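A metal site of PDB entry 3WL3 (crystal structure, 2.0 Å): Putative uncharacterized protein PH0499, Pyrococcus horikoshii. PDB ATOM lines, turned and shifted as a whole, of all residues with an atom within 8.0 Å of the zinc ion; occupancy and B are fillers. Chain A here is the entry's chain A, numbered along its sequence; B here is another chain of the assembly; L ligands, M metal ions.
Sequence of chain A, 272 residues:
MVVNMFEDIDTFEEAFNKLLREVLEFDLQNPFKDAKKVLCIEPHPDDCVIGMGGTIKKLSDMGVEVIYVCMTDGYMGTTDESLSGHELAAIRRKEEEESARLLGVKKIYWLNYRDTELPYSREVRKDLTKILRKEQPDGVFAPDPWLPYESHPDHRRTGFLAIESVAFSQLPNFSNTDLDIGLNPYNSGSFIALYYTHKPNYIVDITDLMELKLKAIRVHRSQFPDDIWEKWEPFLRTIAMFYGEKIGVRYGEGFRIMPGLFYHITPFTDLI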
ATOM      1  N   GLU A  42       8.523  -8.203 -33.847  1.00  0.00           N
ATOM      2  CA  GLU A  42       7.819  -7.544 -32.710  1.00  0.00           C
ATOM      3  C   GLU A  42       6.898  -8.513 -31.908  1.00  0.00           C
ATOM      4  O   GLU A  42       6.307  -9.443 -32.436  1.00  0.00           O
ATOM      5  CB  GLU A  42       7.051  -6.309 -33.185  1.00  0.00           C
ATOM      6  CG  GLU A  42       5.827  -6.681 -34.080  1.00  0.00           C
ATOM      7  CD  GLU A  42       5.132  -5.521 -34.783  1.00  0.00           C
ATOM      8  OE1 GLU A  42       5.304  -4.344 -34.457  1.00  0.00           O
ATOM      9  OE2 GLU A  42       4.395  -5.818 -35.729  1.00  0.00           O
ATOM     10  N   PRO A  43       6.869  -8.388 -30.577  1.00  0.00           N
ATOM     11  CA  PRO A  43       5.991  -9.330 -29.838  1.00  0.00           C
ATOM     12  C   PRO A  43       4.526  -9.069 -30.193  1.00  0.00           C
ATOM     13  O   PRO A  43       3.773 -10.003 -30.475  1.00  0.00           O
ATOM     14  CB  PRO A  43       6.234  -8.942 -28.362  1.00  0.00           C
ATOM     15  CG  PRO A  43       7.692  -8.328 -28.339  1.00  0.00           C
ATOM     16  CD  PRO A  43       7.921  -7.771 -29.751  1.00  0.00           C
ATOM     17  N   HIS A  44       4.165  -7.797 -30.201  1.00  0.00           N
ATOM     18  CA  HIS A  44       2.832  -7.335 -30.504  1.00  0.00           C
ATOM     19  C   HIS A  44       2.792  -6.352 -31.657  1.00  0.00           C
ATOM     20  O   HIS A  44       3.810  -5.736 -31.976  1.00  0.00           O
ATOM     21  CB  HIS A  44       2.237  -6.652 -29.265  1.00  0.00           C
ATOM     22  CG  HIS A  44       2.364  -7.488 -28.017  1.00  0.00           C
ATOM     23  ND1 HIS A  44       3.245  -7.185 -27.010  1.00  0.00           N
ATOM     24  CD2 HIS A  44       1.777  -8.642 -27.652  1.00  0.00           C
ATOM     25  CE1 HIS A  44       3.178  -8.103 -26.064  1.00  0.00           C
ATOM     26  NE2 HIS A  44       2.278  -8.996 -26.425  1.00  0.00           N
ATOM     27  N   PRO A  45       1.584  -6.147 -32.223  1.00  0.00           N
ATOM     28  CA  PRO A  45       1.444  -5.115 -33.235  1.00  0.00           C
ATOM     29  C   PRO A  45       1.554  -3.751 -32.547  1.00  0.00           C
ATOM     30  O   PRO A  45       0.985  -3.561 -31.424  1.00  0.00           O
ATOM     31  CB  PRO A  45       0.064  -5.381 -33.872  1.00  0.00           C
ATOM     32  CG  PRO A  45      -0.680  -6.233 -32.851  1.00  0.00           C
ATOM     33  CD  PRO A  45       0.358  -6.977 -32.090  1.00  0.00           C
ATOM     34  N   ASP A  46       2.345  -2.890 -33.182  1.00  0.00           N
ATOM     35  CA  ASP A  46       2.894  -1.620 -32.672  1.00  0.00           C
ATOM     36  C   ASP A  46       4.328  -1.719 -32.141  1.00  0.00           C
ATOM     37  O   ASP A  46       4.977  -0.722 -32.058  1.00  0.00           O
ATOM     38  CB  ASP A  46       2.010  -0.847 -31.666  1.00  0.00           C
ATOM     39  CG  ASP A  46       1.981  -1.493 -30.244  1.00  0.00           C
ATOM     40  OD1 ASP A  46       2.903  -2.302 -29.919  1.00  0.00           O
ATOM     41  OD2 ASP A  46       1.026  -1.167 -29.449  1.00  0.00           O
ATOM     42  N   ASP A  47       4.821  -2.863 -31.705  1.00  0.00           N
ATOM     43  CA  ASP A  47       6.137  -2.793 -31.031  1.00  0.00           C
ATOM     44  C   ASP A  47       7.267  -2.358 -31.940  1.00  0.00           C
ATOM     45  O   ASP A  47       8.159  -1.643 -31.491  1.00  0.00           O
ATOM     46  CB  ASP A  47       6.520  -4.105 -30.333  1.00  0.00           C
ATOM     47  CG  ASP A  47       5.862  -4.237 -28.983  1.00  0.00           C
ATOM     48  OD1 ASP A  47       5.823  -3.239 -28.262  1.00  0.00           O
ATOM     49  OD2 ASP A  47       5.359  -5.310 -28.677  1.00  0.00           O
ATOM     50  N   CYS A  48       7.253  -2.763 -33.214  1.00  0.00           N
ATOM     51  CA  CYS A  48       8.302  -2.306 -34.141  1.00  0.00           C
ATOM     52  C   CYS A  48       8.297  -0.799 -34.221  1.00  0.00           C
ATOM     53  O   CYS A  48       9.363  -0.160 -34.127  1.00  0.00           O
ATOM     54  CB  CYS A  48       8.126  -2.894 -35.551  1.00  0.00           C
ATOM     55  SG  CYS A  48       8.691  -4.579 -35.752  1.00  0.00           S
ATOM     56  N   ILE A  50       7.048   1.515 -32.065  1.00  0.00           N
ATOM     57  CA  ILE A  50       7.397   2.152 -30.835  1.00  0.00           C
ATOM     58  C   ILE A  50       8.907   1.981 -30.500  1.00  0.00           C
ATOM     59  O   ILE A  50       9.555   2.895 -30.042  1.00  0.00           O
ATOM     60  CB  ILE A  50       6.556   1.528 -29.715  1.00  0.00           C
ATOM     61  CG1 ILE A  50       5.110   2.094 -29.788  1.00  0.00           C
ATOM     62  CG2 ILE A  50       7.198   1.865 -28.422  1.00  0.00           C
ATOM     63  CD1 ILE A  50       4.123   1.132 -29.127  1.00  0.00           C
ATOM     64  N   THR A  72       2.491 -12.115 -32.033  1.00  0.00           N
ATOM     65  CA  THR A  72       1.112 -12.323 -31.517  1.00  0.00           C
ATOM     66  C   THR A  72       0.108 -11.469 -32.199  1.00  0.00           C
ATOM     67  O   THR A  72       0.480 -10.668 -33.026  1.00  0.00           O
ATOM     68  CB  THR A  72       0.973 -12.081 -30.008  1.00  0.00           C
ATOM     69  OG1 THR A  72       1.140 -10.698 -29.702  1.00  0.00           O
ATOM     70  CG2 THR A  72       2.003 -12.889 -29.276  1.00  0.00           C
ATOM     71  N   ARG A  92      -6.430  -4.545 -34.956  1.00  0.00           N
ATOM     72  CA  ARG A  92      -4.971  -4.302 -34.845  1.00  0.00           C
ATOM     73  C   ARG A  92      -4.158  -4.672 -36.093  1.00  0.00           C
ATOM     74  O   ARG A  92      -3.118  -4.068 -36.379  1.00  0.00           O
ATOM     75  CB  ARG A  92      -4.402  -4.943 -33.580  1.00  0.00           C
ATOM     76  CG  ARG A  92      -5.049  -4.344 -32.338  1.00  0.00           C
ATOM     77  CD  ARG A  92      -4.428  -4.787 -31.028  1.00  0.00           C
ATOM     78  NE  ARG A  92      -3.051  -4.297 -30.816  1.00  0.00           N
ATOM     79  CZ  ARG A  92      -2.354  -4.540 -29.700  1.00  0.00           C
ATOM     80  NH1 ARG A  92      -2.910  -5.246 -28.710  1.00  0.00           N
ATOM     81  NH2 ARG A  92      -1.119  -4.020 -29.528  1.00  0.00           N
ATOM     82  N   ASP A 115      -1.764 -13.185 -28.097  1.00  0.00           N
ATOM     83  CA  ASP A 115      -1.337 -12.174 -27.162  1.00  0.00           C
ATOM     84  C   ASP A 115      -1.404 -12.720 -25.726  1.00  0.00           C
ATOM     85  O   ASP A 115      -2.407 -13.246 -25.317  1.00  0.00           O
ATOM     86  CB  ASP A 115      -2.282 -10.987 -27.332  1.00  0.00           C
ATOM     87  CG  ASP A 115      -1.892  -9.775 -26.495  1.00  0.00           C
ATOM     88  OD1 ASP A 115      -0.735  -9.671 -25.987  1.00  0.00           O
ATOM     89  OD2 ASP A 115      -2.779  -8.908 -26.369  1.00  0.00           O
ATOM     90  N   PRO A 143      13.479  -7.430 -29.601  1.00  0.00           N
ATOM     91  CA  PRO A 143      13.629  -6.837 -28.314  1.00  0.00           C
ATOM     92  C   PRO A 143      14.753  -7.563 -27.533  1.00  0.00           C
ATOM     93  O   PRO A 143      14.935  -8.725 -27.680  1.00  0.00           O
ATOM     94  CB  PRO A 143      12.229  -7.088 -27.648  1.00  0.00           C
ATOM     95  CG  PRO A 143      11.272  -7.314 -28.814  1.00  0.00           C
ATOM     96  CD  PRO A 143      12.165  -8.099 -29.738  1.00  0.00           C
ATOM     97  N   GLU A 150      11.372  -5.959 -17.413  1.00  0.00           N
ATOM     98  CA  GLU A 150      10.445  -6.216 -18.521  1.00  0.00           C
ATOM     99  C   GLU A 150       9.486  -7.294 -18.053  1.00  0.00           C
ATOM    100  O   GLU A 150       9.866  -8.430 -17.930  1.00  0.00           O
ATOM    101  CB  GLU A 150      11.150  -6.661 -19.800  1.00  0.00           C
ATOM    102  CG  GLU A 150      10.185  -7.129 -20.831  1.00  0.00           C
ATOM    103  CD  GLU A 150       9.187  -6.034 -21.135  1.00  0.00           C
ATOM    104  OE1 GLU A 150       9.619  -5.015 -21.712  1.00  0.00           O
ATOM    105  OE2 GLU A 150       7.994  -6.151 -20.723  1.00  0.00           O
ATOM    106  N   HIS A 152       6.547  -8.270 -19.377  1.00  0.00           N
ATOM    107  CA  HIS A 152       5.705  -8.933 -20.371  1.00  0.00           C
ATOM    108  C   HIS A 152       6.387 -10.168 -20.956  1.00  0.00           C
ATOM    109  O   HIS A 152       7.311  -9.993 -21.787  1.00  0.00           O
ATOM    110  CB  HIS A 152       5.328  -7.972 -21.521  1.00  0.00           C
ATOM    111  CG  HIS A 152       4.064  -8.359 -22.240  1.00  0.00           C
ATOM    112  ND1 HIS A 152       3.826  -9.646 -22.700  1.00  0.00           N
ATOM    113  CD2 HIS A 152       2.962  -7.628 -22.560  1.00  0.00           C
ATOM    114  CE1 HIS A 152       2.631  -9.696 -23.266  1.00  0.00           C
ATOM    115  NE2 HIS A 152       2.078  -8.488 -23.193  1.00  0.00           N
ATOM    116  N   ASP A 154       5.720 -12.081 -23.338  1.00  0.00           N
ATOM    117  CA  ASP A 154       5.757 -12.150 -24.775  1.00  0.00           C
ATOM    118  C   ASP A 154       7.024 -11.430 -25.260  1.00  0.00           C
ATOM    119  O   ASP A 154       7.542 -11.755 -26.310  1.00  0.00           O
ATOM    120  CB  ASP A 154       4.553 -11.463 -25.418  1.00  0.00           C
ATOM    121  CG  ASP A 154       3.239 -12.274 -25.324  1.00  0.00           C
ATOM    122  OD1 ASP A 154       2.154 -11.692 -25.610  1.00  0.00           O
ATOM    123  OD2 ASP A 154       3.248 -13.456 -24.949  1.00  0.00           O
ATOM    124  N   HIS A 155       7.426 -10.382 -24.537  1.00  0.00           N
ATOM    125  CA  HIS A 155       8.597  -9.598 -24.900  1.00  0.00           C
ATOM    126  C   HIS A 155       9.870 -10.400 -24.620  1.00  0.00           C
ATOM    127  O   HIS A 155      10.724 -10.555 -25.501  1.00  0.00           O
ATOM    128  CB  HIS A 155       8.630  -8.216 -24.223  1.00  0.00           C
ATOM    129  CG  HIS A 155       7.806  -7.188 -24.912  1.00  0.00           C
ATOM    130  ND1 HIS A 155       8.312  -5.982 -25.331  1.00  0.00           N
ATOM    131  CD2 HIS A 155       6.505  -7.199 -25.294  1.00  0.00           C
ATOM    132  CE1 HIS A 155       7.348  -5.272 -25.897  1.00  0.00           C
ATOM    133  NE2 HIS A 155       6.246  -5.991 -25.893  1.00  0.00           N
ATOM    134  N   THR A 158       9.961 -13.375 -27.123  1.00  0.00           N
ATOM    135  CA  THR A 158      10.297 -13.044 -28.525  1.00  0.00           C
ATOM    136  C   THR A 158      11.825 -12.783 -28.710  1.00  0.00           C
ATOM    137  O   THR A 158      12.472 -13.091 -29.767  1.00  0.00           O
ATOM    138  CB  THR A 158       9.605 -11.769 -28.847  1.00  0.00           C
ATOM    139  OG1 THR A 158       8.179 -12.012 -28.904  1.00  0.00           O
ATOM    140  CG2 THR A 158      10.054 -11.307 -30.113  1.00  0.00           C
ATOM    141  N   TYR A 195      16.497  -3.978 -29.983  1.00  0.00           N
ATOM    142  CA  TYR A 195      15.968  -2.751 -29.500  1.00  0.00           C
ATOM    143  C   TYR A 195      15.326  -2.985 -28.134  1.00  0.00           C
ATOM    144  O   TYR A 195      15.487  -4.068 -27.569  1.00  0.00           O
ATOM    145  CB  TYR A 195      14.979  -2.081 -30.470  1.00  0.00           C
ATOM    146  CG  TYR A 195      13.834  -2.923 -30.781  1.00  0.00           C
ATOM    147  CD1 TYR A 195      13.940  -3.928 -31.740  1.00  0.00           C
ATOM    148  CD2 TYR A 195      12.565  -2.711 -30.144  1.00  0.00           C
ATOM    149  CE1 TYR A 195      12.804  -4.724 -32.072  1.00  0.00           C
ATOM    150  CE2 TYR A 195      11.483  -3.504 -30.450  1.00  0.00           C
ATOM    151  CZ  TYR A 195      11.591  -4.470 -31.441  1.00  0.00           C
ATOM    152  OH  TYR A 195      10.529  -5.249 -31.783  1.00  0.00           O
ATOM    153  N   TYR A 196      14.660  -1.937 -27.616  1.00  0.00           N
ATOM    154  CA  TYR A 196      14.171  -1.911 -26.242  1.00  0.00           C
ATOM    155  C   TYR A 196      15.269  -2.360 -25.282  1.00  0.00           C
ATOM    156  O   TYR A 196      15.121  -3.368 -24.537  1.00  0.00           O
ATOM    157  CB  TYR A 196      12.997  -2.865 -26.078  1.00  0.00           C
ATOM    158  CG  TYR A 196      11.629  -2.454 -26.697  1.00  0.00           C
ATOM    159  CD1 TYR A 196      11.264  -1.126 -26.841  1.00  0.00           C
ATOM    160  CD2 TYR A 196      10.731  -3.440 -27.110  1.00  0.00           C
ATOM    161  CE1 TYR A 196      10.012  -0.770 -27.342  1.00  0.00           C
ATOM    162  CE2 TYR A 196       9.482  -3.078 -27.633  1.00  0.00           C
ATOM    163  CZ  TYR A 196       9.127  -1.767 -27.719  1.00  0.00           C
ATOM    164  OH  TYR A 196       7.880  -1.423 -28.259  1.00  0.00           O
ATOM    165  N   TRP A 232       1.512   8.383 -22.530  1.00  0.00           N
ATOM    166  CA  TRP A 232       2.383   7.630 -23.436  1.00  0.00           C
ATOM    167  C   TRP A 232       3.301   8.488 -24.296  1.00  0.00           C
ATOM    168  O   TRP A 232       4.486   8.116 -24.555  1.00  0.00           O
ATOM    169  CB  TRP A 232       1.625   6.543 -24.200  1.00  0.00           C
ATOM    170  CG  TRP A 232       1.719   5.183 -23.480  1.00  0.00           C
ATOM    171  CD1 TRP A 232       1.023   4.807 -22.342  1.00  0.00           C
ATOM    172  CD2 TRP A 232       2.596   4.086 -23.778  1.00  0.00           C
ATOM    173  NE1 TRP A 232       1.417   3.539 -21.955  1.00  0.00           N
ATOM    174  CE2 TRP A 232       2.360   3.064 -22.817  1.00  0.00           C
ATOM    175  CE3 TRP A 232       3.567   3.867 -24.756  1.00  0.00           C
ATOM    176  CZ2 TRP A 232       3.052   1.847 -22.811  1.00  0.00           C
ATOM    177  CZ3 TRP A 232       4.247   2.654 -24.754  1.00  0.00           C
ATOM    178  CH2 TRP A 232       3.998   1.662 -23.779  1.00  0.00           C
ATOM    179  N   HIS B 264       7.700  -2.233 -18.359  1.00  0.00           N
ATOM    180  CA  HIS B 264       7.603  -2.614 -19.740  1.00  0.00           C
ATOM    181  C   HIS B 264       8.428  -1.619 -20.600  1.00  0.00           C
ATOM    182  O   HIS B 264       8.244  -0.403 -20.500  1.00  0.00           O
ATOM    183  CB  HIS B 264       6.090  -2.619 -20.166  1.00  0.00           C
ATOM    184  CG  HIS B 264       5.838  -3.250 -21.507  1.00  0.00           C
ATOM    185  ND1 HIS B 264       6.293  -4.509 -21.840  1.00  0.00           N
ATOM    186  CD2 HIS B 264       5.185  -2.779 -22.608  1.00  0.00           C
ATOM    187  CE1 HIS B 264       5.927  -4.793 -23.082  1.00  0.00           C
ATOM    188  NE2 HIS B 264       5.240  -3.763 -23.564  1.00  0.00           N
ATOM    189  N   ILE B 265       9.371  -2.153 -21.392  1.00  0.00           N
ATOM    190  CA  ILE B 265      10.237  -1.407 -22.348  1.00  0.00           C
ATOM    191  C   ILE B 265      10.979  -0.235 -21.784  1.00  0.00           C
ATOM    192  O   ILE B 265      11.464   0.643 -22.514  1.00  0.00           O
ATOM    193  CB  ILE B 265       9.435  -0.981 -23.644  1.00  0.00           C
ATOM    194  CG1 ILE B 265       8.414   0.134 -23.332  1.00  0.00           C
ATOM    195  CG2 ILE B 265       8.687  -2.181 -24.215  1.00  0.00           C
ATOM    196  CD1 ILE B 265       7.818   0.864 -24.636  1.00  0.00           C
HETATM  197  P1  LIG L   1       3.191  -2.946 -26.340  1.00  0.00           P
HETATM  198  O1  LIG L   1       3.948  -4.136 -25.825  1.00  0.00           O
HETATM  199  O2  LIG L   1       2.173  -2.507 -25.274  1.00  0.00           O
HETATM  200  O3  LIG L   1       2.503  -3.179 -27.672  1.00  0.00           O
HETATM  201  O4  LIG L   1       4.255  -1.916 -26.584  1.00  0.00           O
HETATM  202 ZN    ZN M   1       4.481  -5.536 -26.845  1.00  0.00          ZN
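His 264 of chain B touches the zinc ion (NE2 to ZN, 3.8 Å).
O1 of the ligand is bound to the zinc ion (1.8 Å).
The zinc ion is bound by OD2 of Asp 47, at 2.0 Å.
A ring nitrogen (NE2) of His 155 is bound to the zinc ion (2.1 Å).
The zinc ion is bound by ND1 of His 44, at 2.1 Å.
The zinc ion has four donor atoms within binding distance.
The side-chain carboxylate (OD1) of Asp 47 is in hydrogen-bond range of the side-chain hydroxyl (OH) of Tyr 196, at 2.7 Å.
The side-chain carboxylate of Glu 42 is in hydrogen-bond range of the backbone NH of Asp 47 (3.2 Å).
A ring nitrogen (NE2) of His 155 sits close to a ring nitrogen (NE2) of His 264 of chain B (3.4 Å).
NE2 of His 44 lies close to NE2 of His 152.
The side-chain carboxylate of Asp 154 lies within hydrogen-bond range of a ring nitrogen (NE2) of His 44 (2.8 Å).
A ring nitrogen (NE2) of His 44 sits at hydrogen-bond distance from the side-chain carboxylate (OD1) of Asp 115 (3.1 Å).
OE2 of Glu 150 lies within hydrogen-bond range of ND1 of His 264 of chain B, at 2.6 Å.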
